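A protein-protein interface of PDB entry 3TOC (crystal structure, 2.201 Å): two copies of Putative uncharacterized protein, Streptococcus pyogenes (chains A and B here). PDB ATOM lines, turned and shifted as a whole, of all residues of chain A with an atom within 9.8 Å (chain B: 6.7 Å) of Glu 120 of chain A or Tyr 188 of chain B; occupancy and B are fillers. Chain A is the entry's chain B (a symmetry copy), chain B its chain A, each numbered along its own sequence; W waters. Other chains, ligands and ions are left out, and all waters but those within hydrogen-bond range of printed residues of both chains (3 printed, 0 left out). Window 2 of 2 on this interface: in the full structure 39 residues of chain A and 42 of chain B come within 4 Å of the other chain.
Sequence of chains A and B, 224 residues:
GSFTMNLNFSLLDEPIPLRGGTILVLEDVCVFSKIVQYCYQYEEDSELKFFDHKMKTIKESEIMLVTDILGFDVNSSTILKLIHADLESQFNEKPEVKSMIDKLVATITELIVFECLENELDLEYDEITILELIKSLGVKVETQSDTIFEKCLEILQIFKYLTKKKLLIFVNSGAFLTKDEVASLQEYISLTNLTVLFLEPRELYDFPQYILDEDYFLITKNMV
The side-chain amide nitrogen of Asn 119 of chain A lies within hydrogen-bond range of the side-chain carboxylate of Asp 86 of chain B (3.0 Å).
O of Glu 115 of chain A lies within hydrogen-bond range of NE2 of Gln 90 of chain B (2.8 Å).
The side-chain amide oxygen (OE1) of Gln 90 of chain B lies within hydrogen-bond range of the side-chain amide nitrogen (ND2) of Asn 119 of chain A (2.8 Å).
OH of Tyr 188 of chain B sits at hydrogen-bond distance from OE2 of Glu 120 of chain A (2.5 Å).
The side-chain carboxylate (OD2) of Asp 86 of chain B lies within hydrogen-bond range of the side-chain hydroxyl (OH) of Tyr 161 of chain B.
The backbone carbonyl oxygen (O) of Tyr 188 of chain B sits at hydrogen-bond distance from the side-chain hydroxyl (OG1) of Thr 192 of chain B.
OD1 of Asn 119 of chain A sits at hydrogen-bond distance from N of Leu 121 of chain A (3.0 Å).
Among the printed residues, merely in contact across the chains: Asn 119 of chain A with Tyr 161 of chain B (3.5 Å), Glu 120 of chain A with Gln 157 of chain B (3.7 Å), Leu 121 of chain A with Gln 157 of chain B (3.5 Å) and Leu 121 of chain A with Tyr 161 of chain B (3.9 Å).
Of chain B, only Gln 157 and Tyr 188 come within 4 Å of Glu 120 of chain A.
Tyr 188 of chain B touches one residue of chain A.
Gln 157 of chain B touches just these residues of chain A: Glu 120 and Leu 121.
No residue of chain A comes within 4 Å of Ile 189 of chain B.
No residue of chain A comes within 4 Å of Thr 192 of chain B.
Printed residues of chain A within 4 Å of Tyr 161 of chain B: Asn 119 (3.5 Å) and Leu 121 (3.9 Å).
Printed residues of chain A within 4 Å of Asp 86 of chain B: Asn 119.
Of the printed residues of chain A, Gln 90 of chain B touches Glu 115 (2.8 Å) and Asn 119 (2.8 Å).
The nearest residue of chain A that does not touch Tyr 188 of chain B is Leu 121 of chain A (7.0 Å).
The nearest printed residue of chain A that does not touch Tyr 161 of chain B is Glu 120 of chain A (6.4 Å).
Of the 20 printed residues of chain B, 5 touch a printed residue of chain A.
Hydrophobic or aromatic side chains of chain B that line the printed part of chain A: Tyr 161 and Tyr 188.
Printed residues of chain A that touch a printed residue of chain B: Glu 115, Asn 119, Glu 120 and Leu 121.
Hydrophobic or aromatic side chains of chain A that line the printed part of chain B: Leu 121.
No position is printed for both chains.
Of the 8 pairs that touch across the chains among the printed residues, none has its exchanged pair printed and touching as well.
Water W2 lies within hydrogen-bond range of OD1 of Asn 119 of chain A (2.7 Å) and OH of Tyr 161 of chain B (2.9 Å).
Water W3 bridges OE1 of Gln 157 of chain B (2.9 Å) and N of Asp 122 of chain A (2.9 Å).
Water W1 bridges O of Gln 157 of chain B and OE2 of Glu 120 of chain A.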
ATOM      1  N   VAL A 113     -27.126  -0.176 -16.373  1.00  0.00           N
ATOM      2  CA  VAL A 113     -25.683  -0.153 -16.198  1.00  0.00           C
ATOM      3  C   VAL A 113     -25.133  -1.570 -16.058  1.00  0.00           C
ATOM      4  O   VAL A 113     -23.997  -1.849 -16.451  1.00  0.00           O
ATOM      5  CB  VAL A 113     -25.269   0.675 -14.968  1.00  0.00           C
ATOM      6  CG1 VAL A 113     -23.808   0.475 -14.687  1.00  0.00           C
ATOM      7  CG2 VAL A 113     -25.538   2.136 -15.228  1.00  0.00           C
ATOM      8  N   PHE A 114     -25.947  -2.470 -15.518  1.00  0.00           N
ATOM      9  CA  PHE A 114     -25.530  -3.851 -15.393  1.00  0.00           C
ATOM     10  C   PHE A 114     -25.235  -4.391 -16.779  1.00  0.00           C
ATOM     11  O   PHE A 114     -24.245  -5.066 -16.990  1.00  0.00           O
ATOM     12  CB  PHE A 114     -26.593  -4.717 -14.695  1.00  0.00           C
ATOM     13  CG  PHE A 114     -26.097  -6.092 -14.328  1.00  0.00           C
ATOM     14  CD1 PHE A 114     -25.682  -6.376 -13.036  1.00  0.00           C
ATOM     15  CD2 PHE A 114     -26.044  -7.101 -15.281  1.00  0.00           C
ATOM     16  CE1 PHE A 114     -25.233  -7.642 -12.694  1.00  0.00           C
ATOM     17  CE2 PHE A 114     -25.581  -8.355 -14.959  1.00  0.00           C
ATOM     18  CZ  PHE A 114     -25.179  -8.629 -13.657  1.00  0.00           C
ATOM     19  N   GLU A 115     -26.098  -4.088 -17.729  1.00  0.00           N
ATOM     20  CA  GLU A 115     -25.890  -4.577 -19.083  1.00  0.00           C
ATOM     21  C   GLU A 115     -24.725  -3.835 -19.725  1.00  0.00           C
ATOM     22  O   GLU A 115     -24.074  -4.351 -20.642  1.00  0.00           O
ATOM     23  CB  GLU A 115     -27.167  -4.418 -19.908  1.00  0.00           C
ATOM     24  CG  GLU A 115     -28.356  -5.162 -19.297  1.00  0.00           C
ATOM     25  CD  GLU A 115     -28.046  -6.629 -19.086  1.00  0.00           C
ATOM     26  OE1 GLU A 115     -27.287  -7.186 -19.900  1.00  0.00           O
ATOM     27  OE2 GLU A 115     -28.550  -7.225 -18.114  1.00  0.00           O
ATOM     28  N   CYS A 116     -24.443  -2.634 -19.232  1.00  0.00           N
ATOM     29  CA  CYS A 116     -23.307  -1.887 -19.765  1.00  0.00           C
ATOM     30  C   CYS A 116     -21.979  -2.549 -19.386  1.00  0.00           C
ATOM     31  O   CYS A 116     -21.063  -2.597 -20.197  1.00  0.00           O
ATOM     32  CB  CYS A 116     -23.328  -0.430 -19.305  1.00  0.00           C
ATOM     33  SG  CYS A 116     -24.641   0.562 -20.060  1.00  0.00           S
ATOM     34  N   LEU A 117     -21.897  -3.056 -18.161  1.00  0.00           N
ATOM     35  CA  LEU A 117     -20.692  -3.687 -17.632  1.00  0.00           C
ATOM     36  C   LEU A 117     -20.460  -4.998 -18.337  1.00  0.00           C
ATOM     37  O   LEU A 117     -19.331  -5.356 -18.671  1.00  0.00           O
ATOM     38  CB  LEU A 117     -20.847  -3.935 -16.135  1.00  0.00           C
ATOM     39  CG  LEU A 117     -20.837  -2.629 -15.350  1.00  0.00           C
ATOM     40  CD1 LEU A 117     -21.310  -2.846 -13.938  1.00  0.00           C
ATOM     41  CD2 LEU A 117     -19.450  -2.016 -15.359  1.00  0.00           C
ATOM     42  N   GLU A 118     -21.555  -5.712 -18.552  1.00  0.00           N
ATOM     43  CA  GLU A 118     -21.531  -6.979 -19.244  1.00  0.00           C
ATOM     44  C   GLU A 118     -21.055  -6.760 -20.666  1.00  0.00           C
ATOM     45  O   GLU A 118     -20.426  -7.633 -21.251  1.00  0.00           O
ATOM     46  CB  GLU A 118     -22.932  -7.589 -19.273  1.00  0.00           C
ATOM     47  CG  GLU A 118     -23.459  -8.021 -17.920  1.00  0.00           C
ATOM     48  CD  GLU A 118     -23.283  -9.509 -17.681  1.00  0.00           C
ATOM     49  OE1 GLU A 118     -22.116  -9.954 -17.556  1.00  0.00           O
ATOM     50  OE2 GLU A 118     -24.315 -10.225 -17.636  1.00  0.00           O
ATOM     51  N   ASN A 119     -21.359  -5.593 -21.229  1.00  0.00           N
ATOM     52  CA  ASN A 119     -20.944  -5.291 -22.595  1.00  0.00           C
ATOM     53  C   ASN A 119     -19.410  -5.196 -22.716  1.00  0.00           C
ATOM     54  O   ASN A 119     -18.744  -4.702 -21.802  1.00  0.00           O
ATOM     55  CB  ASN A 119     -21.631  -4.020 -23.101  1.00  0.00           C
ATOM     56  CG  ASN A 119     -21.552  -3.878 -24.606  1.00  0.00           C
ATOM     57  OD1 ASN A 119     -20.552  -3.392 -25.130  1.00  0.00           O
ATOM     58  ND2 ASN A 119     -22.603  -4.302 -25.312  1.00  0.00           N
ATOM     59  N   GLU A 120     -18.859  -5.700 -23.823  1.00  0.00           N
ATOM     60  CA  GLU A 120     -17.408  -5.625 -24.093  1.00  0.00           C
ATOM     61  C   GLU A 120     -16.839  -4.222 -23.950  1.00  0.00           C
ATOM     62  O   GLU A 120     -15.718  -4.035 -23.465  1.00  0.00           O
ATOM     63  CB  GLU A 120     -17.101  -6.083 -25.516  1.00  0.00           C
ATOM     64  CG  GLU A 120     -17.070  -7.583 -25.708  1.00  0.00           C
ATOM     65  CD  GLU A 120     -16.498  -7.956 -27.061  1.00  0.00           C
ATOM     66  OE1 GLU A 120     -15.672  -8.899 -27.126  1.00  0.00           O
ATOM     67  OE2 GLU A 120     -16.871  -7.293 -28.057  1.00  0.00           O
ATOM     68  N   LEU A 121     -17.622  -3.243 -24.399  1.00  0.00           N
ATOM     69  CA  LEU A 121     -17.193  -1.857 -24.439  1.00  0.00           C
ATOM     70  C   LEU A 121     -17.123  -1.229 -23.067  1.00  0.00           C
ATOM     71  O   LEU A 121     -17.977  -1.454 -22.209  1.00  0.00           O
ATOM     72  CB  LEU A 121     -18.159  -1.036 -25.281  1.00  0.00           C
ATOM     73  CG  LEU A 121     -18.098  -1.214 -26.780  1.00  0.00           C
ATOM     74  CD1 LEU A 121     -19.358  -0.654 -27.399  1.00  0.00           C
ATOM     75  CD2 LEU A 121     -16.861  -0.498 -27.292  1.00  0.00           C
ATOM     76  N   ASP A 122     -16.107  -0.407 -22.890  1.00  0.00           N
ATOM     77  CA  ASP A 122     -16.020   0.491 -21.759  1.00  0.00           C
ATOM     78  C   ASP A 122     -17.055   1.612 -21.919  1.00  0.00           C
ATOM     79  O   ASP A 122     -16.803   2.621 -22.600  1.00  0.00           O
ATOM     80  CB  ASP A 122     -14.620   1.089 -21.699  1.00  0.00           C
ATOM     81  CG  ASP A 122     -14.412   1.887 -20.455  1.00  0.00           C
ATOM     82  OD1 ASP A 122     -13.409   2.616 -20.354  1.00  0.00           O
ATOM     83  OD2 ASP A 122     -15.273   1.778 -19.560  1.00  0.00           O
ATOM     84  N   LEU A 123     -18.211   1.433 -21.283  1.00  0.00           N
ATOM     85  CA  LEU A 123     -19.332   2.368 -21.422  1.00  0.00           C
ATOM     86  C   LEU A 123     -19.479   3.263 -20.199  1.00  0.00           C
ATOM     87  O   LEU A 123     -19.357   2.815 -19.066  1.00  0.00           O
ATOM     88  CB  LEU A 123     -20.638   1.603 -21.663  1.00  0.00           C
ATOM     89  CG  LEU A 123     -20.657   0.836 -22.980  1.00  0.00           C
ATOM     90  CD1 LEU A 123     -21.877  -0.033 -23.038  1.00  0.00           C
ATOM     91  CD2 LEU A 123     -20.644   1.806 -24.141  1.00  0.00           C
ATOM     92  N   ASP B  86     -27.935  -2.928 -29.086  1.00  0.00           N
ATOM     93  CA  ASP B  86     -27.264  -4.108 -28.561  1.00  0.00           C
ATOM     94  C   ASP B  86     -27.633  -4.335 -27.106  1.00  0.00           C
ATOM     95  O   ASP B  86     -27.972  -5.443 -26.715  1.00  0.00           O
ATOM     96  CB  ASP B  86     -25.748  -3.960 -28.699  1.00  0.00           C
ATOM     97  CG  ASP B  86     -25.008  -5.254 -28.421  1.00  0.00           C
ATOM     98  OD1 ASP B  86     -25.563  -6.331 -28.755  1.00  0.00           O
ATOM     99  OD2 ASP B  86     -23.879  -5.187 -27.868  1.00  0.00           O
ATOM    100  N   GLN B  90     -29.654  -7.328 -25.121  1.00  0.00           N
ATOM    101  CA  GLN B  90     -29.111  -8.034 -23.964  1.00  0.00           C
ATOM    102  C   GLN B  90     -30.258  -8.394 -22.984  1.00  0.00           C
ATOM    103  O   GLN B  90     -30.224  -9.441 -22.350  1.00  0.00           O
ATOM    104  CB  GLN B  90     -27.965  -7.239 -23.302  1.00  0.00           C
ATOM    105  CG  GLN B  90     -26.612  -7.318 -24.092  1.00  0.00           C
ATOM    106  CD  GLN B  90     -25.478  -6.431 -23.537  1.00  0.00           C
ATOM    107  OE1 GLN B  90     -24.709  -5.843 -24.312  1.00  0.00           O
ATOM    108  NE2 GLN B  90     -25.355  -6.352 -22.207  1.00  0.00           N
ATOM    109  N   LEU B 153      -8.590  -1.131 -28.830  1.00  0.00           N
ATOM    110  CA  LEU B 153      -9.570  -2.142 -28.518  1.00  0.00           C
ATOM    111  C   LEU B 153     -10.975  -1.627 -28.786  1.00  0.00           C
ATOM    112  O   LEU B 153     -11.779  -2.305 -29.436  1.00  0.00           O
ATOM    113  CB  LEU B 153      -9.431  -2.589 -27.066  1.00  0.00           C
ATOM    114  CG  LEU B 153      -8.861  -3.983 -26.855  1.00  0.00           C
ATOM    115  CD1 LEU B 153      -8.782  -4.242 -25.370  1.00  0.00           C
ATOM    116  CD2 LEU B 153      -9.729  -5.025 -27.537  1.00  0.00           C
ATOM    117  N   LEU B 156     -11.795  -1.566 -32.466  1.00  0.00           N
ATOM    118  CA  LEU B 156     -12.087  -2.936 -32.886  1.00  0.00           C
ATOM    119  C   LEU B 156     -13.515  -3.316 -32.486  1.00  0.00           C
ATOM    120  O   LEU B 156     -14.244  -3.956 -33.257  1.00  0.00           O
ATOM    121  CB  LEU B 156     -11.093  -3.924 -32.270  1.00  0.00           C
ATOM    122  CG  LEU B 156      -9.637  -3.850 -32.739  1.00  0.00           C
ATOM    123  CD1 LEU B 156      -8.800  -4.901 -32.014  1.00  0.00           C
ATOM    124  CD2 LEU B 156      -9.573  -4.062 -34.214  1.00  0.00           C
ATOM    125  N   GLN B 157     -13.912  -2.899 -31.286  1.00  0.00           N
ATOM    126  CA  GLN B 157     -15.195  -3.302 -30.726  1.00  0.00           C
ATOM    127  C   GLN B 157     -16.386  -2.578 -31.371  1.00  0.00           C
ATOM    128  O   GLN B 157     -17.464  -3.155 -31.507  1.00  0.00           O
ATOM    129  CB  GLN B 157     -15.189  -3.152 -29.201  1.00  0.00           C
ATOM    130  CG  GLN B 157     -14.261  -4.150 -28.506  1.00  0.00           C
ATOM    131  CD  GLN B 157     -13.962  -3.793 -27.068  1.00  0.00           C
ATOM    132  OE1 GLN B 157     -14.168  -2.660 -26.642  1.00  0.00           O
ATOM    133  NE2 GLN B 157     -13.472  -4.769 -26.304  1.00  0.00           N
ATOM    134  N   ILE B 158     -16.193  -1.336 -31.796  1.00  0.00           N
ATOM    135  CA  ILE B 158     -17.257  -0.659 -32.523  1.00  0.00           C
ATOM    136  C   ILE B 158     -17.236  -1.124 -33.970  1.00  0.00           C
ATOM    137  O   ILE B 158     -18.277  -1.253 -34.611  1.00  0.00           O
ATOM    138  CB  ILE B 158     -17.214   0.889 -32.368  1.00  0.00           C
ATOM    139  CG1 ILE B 158     -15.968   1.495 -33.005  1.00  0.00           C
ATOM    140  CG2 ILE B 158     -17.291   1.265 -30.900  1.00  0.00           C
ATOM    141  CD1 ILE B 158     -16.153   1.869 -34.468  1.00  0.00           C
ATOM    142  N   LYS B 160     -16.864  -4.122 -35.026  1.00  0.00           N
ATOM    143  CA  LYS B 160     -17.677  -5.333 -35.160  1.00  0.00           C
ATOM    144  C   LYS B 160     -19.161  -5.037 -35.395  1.00  0.00           C
ATOM    145  O   LYS B 160     -19.867  -5.823 -36.027  1.00  0.00           O
ATOM    146  CB  LYS B 160     -17.523  -6.243 -33.936  1.00  0.00           C
ATOM    147  CG  LYS B 160     -18.361  -7.512 -34.024  1.00  0.00           C
ATOM    148  CD  LYS B 160     -18.362  -8.311 -32.718  1.00  0.00           C
ATOM    149  CE  LYS B 160     -19.297  -7.720 -31.653  1.00  0.00           C
ATOM    150  NZ  LYS B 160     -20.737  -8.122 -31.808  1.00  0.00           N
ATOM    151  N   TYR B 161     -19.637  -3.916 -34.867  1.00  0.00           N
ATOM    152  CA  TYR B 161     -21.032  -3.538 -35.041  1.00  0.00           C
ATOM    153  C   TYR B 161     -21.327  -3.165 -36.478  1.00  0.00           C
ATOM    154  O   TYR B 161     -22.443  -3.362 -36.958  1.00  0.00           O
ATOM    155  CB  TYR B 161     -21.388  -2.348 -34.154  1.00  0.00           C
ATOM    156  CG  TYR B 161     -21.653  -2.690 -32.710  1.00  0.00           C
ATOM    157  CD1 TYR B 161     -22.624  -3.609 -32.358  1.00  0.00           C
ATOM    158  CD2 TYR B 161     -20.949  -2.067 -31.696  1.00  0.00           C
ATOM    159  CE1 TYR B 161     -22.880  -3.906 -31.025  1.00  0.00           C
ATOM    160  CE2 TYR B 161     -21.200  -2.348 -30.381  1.00  0.00           C
ATOM    161  CZ  TYR B 161     -22.155  -3.266 -30.050  1.00  0.00           C
ATOM    162  OH  TYR B 161     -22.366  -3.522 -28.726  1.00  0.00           O
ATOM    163  N   ALA B 183      -0.178  -8.519 -29.224  1.00  0.00           N
ATOM    164  CA  ALA B 183      -0.735  -9.830 -28.907  1.00  0.00           C
ATOM    165  C   ALA B 183      -2.232  -9.767 -28.551  1.00  0.00           C
ATOM    166  O   ALA B 183      -3.049 -10.431 -29.198  1.00  0.00           O
ATOM    167  CB  ALA B 183       0.064 -10.499 -27.795  1.00  0.00           C
ATOM    168  N   SER B 184      -2.600  -8.962 -27.549  1.00  0.00           N
ATOM    169  CA  SER B 184      -4.012  -8.847 -27.144  1.00  0.00           C
ATOM    170  C   SER B 184      -4.944  -8.427 -28.279  1.00  0.00           C
ATOM    171  O   SER B 184      -6.054  -8.944 -28.373  1.00  0.00           O
ATOM    172  CB  SER B 184      -4.198  -7.891 -25.960  1.00  0.00           C
ATOM    173  OG  SER B 184      -3.576  -8.395 -24.789  1.00  0.00           O
ATOM    174  N   LEU B 185      -4.506  -7.486 -29.126  1.00  0.00           N
ATOM    175  CA  LEU B 185      -5.321  -7.045 -30.260  1.00  0.00           C
ATOM    176  C   LEU B 185      -5.504  -8.166 -31.297  1.00  0.00           C
ATOM    177  O   LEU B 185      -6.627  -8.452 -31.716  1.00  0.00           O
ATOM    178  CB  LEU B 185      -4.745  -5.789 -30.935  1.00  0.00           C
ATOM    179  CG  LEU B 185      -4.624  -4.485 -30.138  1.00  0.00           C
ATOM    180  CD1 LEU B 185      -4.067  -3.398 -31.056  1.00  0.00           C
ATOM    181  CD2 LEU B 185      -5.957  -4.036 -29.515  1.00  0.00           C
ATOM    182  N   GLN B 186      -4.410  -8.807 -31.708  1.00  0.00           N
ATOM    183  CA  GLN B 186      -4.516  -9.929 -32.637  1.00  0.00           C
ATOM    184  C   GLN B 186      -5.507 -10.985 -32.103  1.00  0.00           C
ATOM    185  O   GLN B 186      -6.341 -11.508 -32.842  1.00  0.00           O
ATOM    186  CB  GLN B 186      -3.139 -10.559 -32.891  1.00  0.00           C
ATOM    187  CG  GLN B 186      -2.064  -9.598 -33.396  1.00  0.00           C
ATOM    188  CD  GLN B 186      -2.105  -9.392 -34.893  1.00  0.00           C
ATOM    189  OE1 GLN B 186      -3.077  -8.872 -35.433  1.00  0.00           O
ATOM    190  NE2 GLN B 186      -1.044  -9.802 -35.572  1.00  0.00           N
ATOM    191  N   GLU B 187      -5.415 -11.285 -30.814  1.00  0.00           N
ATOM    192  CA  GLU B 187      -6.295 -12.269 -30.185  1.00  0.00           C
ATOM    193  C   GLU B 187      -7.782 -11.866 -30.275  1.00  0.00           C
ATOM    194  O   GLU B 187      -8.646 -12.680 -30.624  1.00  0.00           O
ATOM    195  CB  GLU B 187      -5.860 -12.478 -28.730  1.00  0.00           C
ATOM    196  CG  GLU B 187      -6.588 -13.573 -27.975  1.00  0.00           C
ATOM    197  CD  GLU B 187      -5.925 -13.869 -26.638  1.00  0.00           C
ATOM    198  OE1 GLU B 187      -4.739 -13.494 -26.472  1.00  0.00           O
ATOM    199  OE2 GLU B 187      -6.584 -14.471 -25.757  1.00  0.00           O
ATOM    200  N   TYR B 188      -8.078 -10.606 -29.975  1.00  0.00           N
ATOM    201  CA  TYR B 188      -9.445 -10.122 -30.073  1.00  0.00           C
ATOM    202  C   TYR B 188      -9.979 -10.180 -31.507  1.00  0.00           C
ATOM    203  O   TYR B 188     -11.125 -10.568 -31.742  1.00  0.00           O
ATOM    204  CB  TYR B 188      -9.572  -8.705 -29.527  1.00  0.00           C
ATOM    205  CG  TYR B 188     -11.003  -8.233 -29.560  1.00  0.00           C
ATOM    206  CD1 TYR B 188     -11.877  -8.536 -28.519  1.00  0.00           C
ATOM    207  CD2 TYR B 188     -11.491  -7.530 -30.647  1.00  0.00           C
ATOM    208  CE1 TYR B 188     -13.192  -8.130 -28.552  1.00  0.00           C
ATOM    209  CE2 TYR B 188     -12.805  -7.117 -30.691  1.00  0.00           C
ATOM    210  CZ  TYR B 188     -13.653  -7.420 -29.641  1.00  0.00           C
ATOM    211  OH  TYR B 188     -14.965  -7.004 -29.693  1.00  0.00           O
ATOM    212  N   ILE B 189      -9.135  -9.796 -32.461  1.00  0.00           N
ATOM    213  CA  ILE B 189      -9.492  -9.834 -33.875  1.00  0.00           C
ATOM    214  C   ILE B 189      -9.948 -11.227 -34.304  1.00  0.00           C
ATOM    215  O   ILE B 189     -10.995 -11.382 -34.930  1.00  0.00           O
ATOM    216  CB  ILE B 189      -8.316  -9.349 -34.749  1.00  0.00           C
ATOM    217  CG1 ILE B 189      -8.222  -7.823 -34.684  1.00  0.00           C
ATOM    218  CG2 ILE B 189      -8.467  -9.829 -36.187  1.00  0.00           C
ATOM    219  CD1 ILE B 189      -6.850  -7.280 -35.030  1.00  0.00           C
ATOM    220  N   SER B 190      -9.168 -12.236 -33.939  1.00  0.00           N
ATOM    221  CA  SER B 190      -9.468 -13.608 -34.326  1.00  0.00           C
ATOM    222  C   SER B 190     -10.731 -14.123 -33.640  1.00  0.00           C
ATOM    223  O   SER B 190     -11.542 -14.827 -34.255  1.00  0.00           O
ATOM    224  CB  SER B 190      -8.277 -14.524 -34.024  1.00  0.00           C
ATOM    225  OG  SER B 190      -8.528 -15.850 -34.467  1.00  0.00           O
ATOM    226  N   LEU B 191     -10.897 -13.759 -32.371  1.00  0.00           N
ATOM    227  CA  LEU B 191     -12.025 -14.225 -31.582  1.00  0.00           C
ATOM    228  C   LEU B 191     -13.327 -13.667 -32.137  1.00  0.00           C
ATOM    229  O   LEU B 191     -14.387 -14.277 -32.002  1.00  0.00           O
ATOM    230  CB  LEU B 191     -11.852 -13.787 -30.127  1.00  0.00           C
ATOM    231  CG  LEU B 191     -12.630 -14.559 -29.057  1.00  0.00           C
ATOM    232  CD1 LEU B 191     -11.802 -15.753 -28.571  1.00  0.00           C
ATOM    233  CD2 LEU B 191     -13.003 -13.634 -27.900  1.00  0.00           C
ATOM    234  N   THR B 192     -13.222 -12.503 -32.771  1.00  0.00           N
ATOM    235  CA  THR B 192     -14.362 -11.742 -33.260  1.00  0.00           C
ATOM    236  C   THR B 192     -14.524 -11.861 -34.772  1.00  0.00           C
ATOM    237  O   THR B 192     -15.409 -11.255 -35.366  1.00  0.00           O
ATOM    238  CB  THR B 192     -14.187 -10.273 -32.887  1.00  0.00           C
ATOM    239  OG1 THR B 192     -14.135 -10.166 -31.461  1.00  0.00           O
ATOM    240  CG2 THR B 192     -15.339  -9.451 -33.391  1.00  0.00           C
ATOM    241  N   ASN B 193     -13.662 -12.646 -35.404  1.00  0.00           N
ATOM    242  CA  ASN B 193     -13.806 -12.889 -36.829  1.00  0.00           C
ATOM    243  C   ASN B 193     -13.741 -11.603 -37.620  1.00  0.00           C
ATOM    244  O   ASN B 193     -14.463 -11.430 -38.601  1.00  0.00           O
ATOM    245  CB  ASN B 193     -15.129 -13.590 -37.103  1.00  0.00           C
ATOM    246  CG  ASN B 193     -15.162 -14.977 -36.525  1.00  0.00           C
ATOM    247  OD1 ASN B 193     -14.157 -15.695 -36.568  1.00  0.00           O
ATOM    248  ND2 ASN B 193     -16.303 -15.364 -35.959  1.00  0.00           N
ATOM    249  N   LEU B 194     -12.888 -10.692 -37.177  1.00  0.00           N
ATOM    250  CA  LEU B 194     -12.663  -9.455 -37.904  1.00  0.00           C
ATOM    251  C   LEU B 194     -11.583  -9.618 -38.956  1.00  0.00           C
ATOM    252  O   LEU B 194     -10.814 -10.583 -38.946  1.00  0.00           O
ATOM    253  CB  LEU B 194     -12.239  -8.348 -36.951  1.00  0.00           C
ATOM    254  CG  LEU B 194     -13.318  -7.991 -35.956  1.00  0.00           C
ATOM    255  CD1 LEU B 194     -12.816  -6.851 -35.078  1.00  0.00           C
ATOM    256  CD2 LEU B 194     -14.580  -7.627 -36.730  1.00  0.00           C
HETATM  257  O   HOH W   1     -18.710  -5.301 -29.825  1.00  0.00           O
HETATM  258  O   HOH W   2     -19.829  -4.396 -27.548  1.00  0.00           O
HETATM  259  O   HOH W   3     -13.600  -1.160 -24.222  1.00  0.00           O
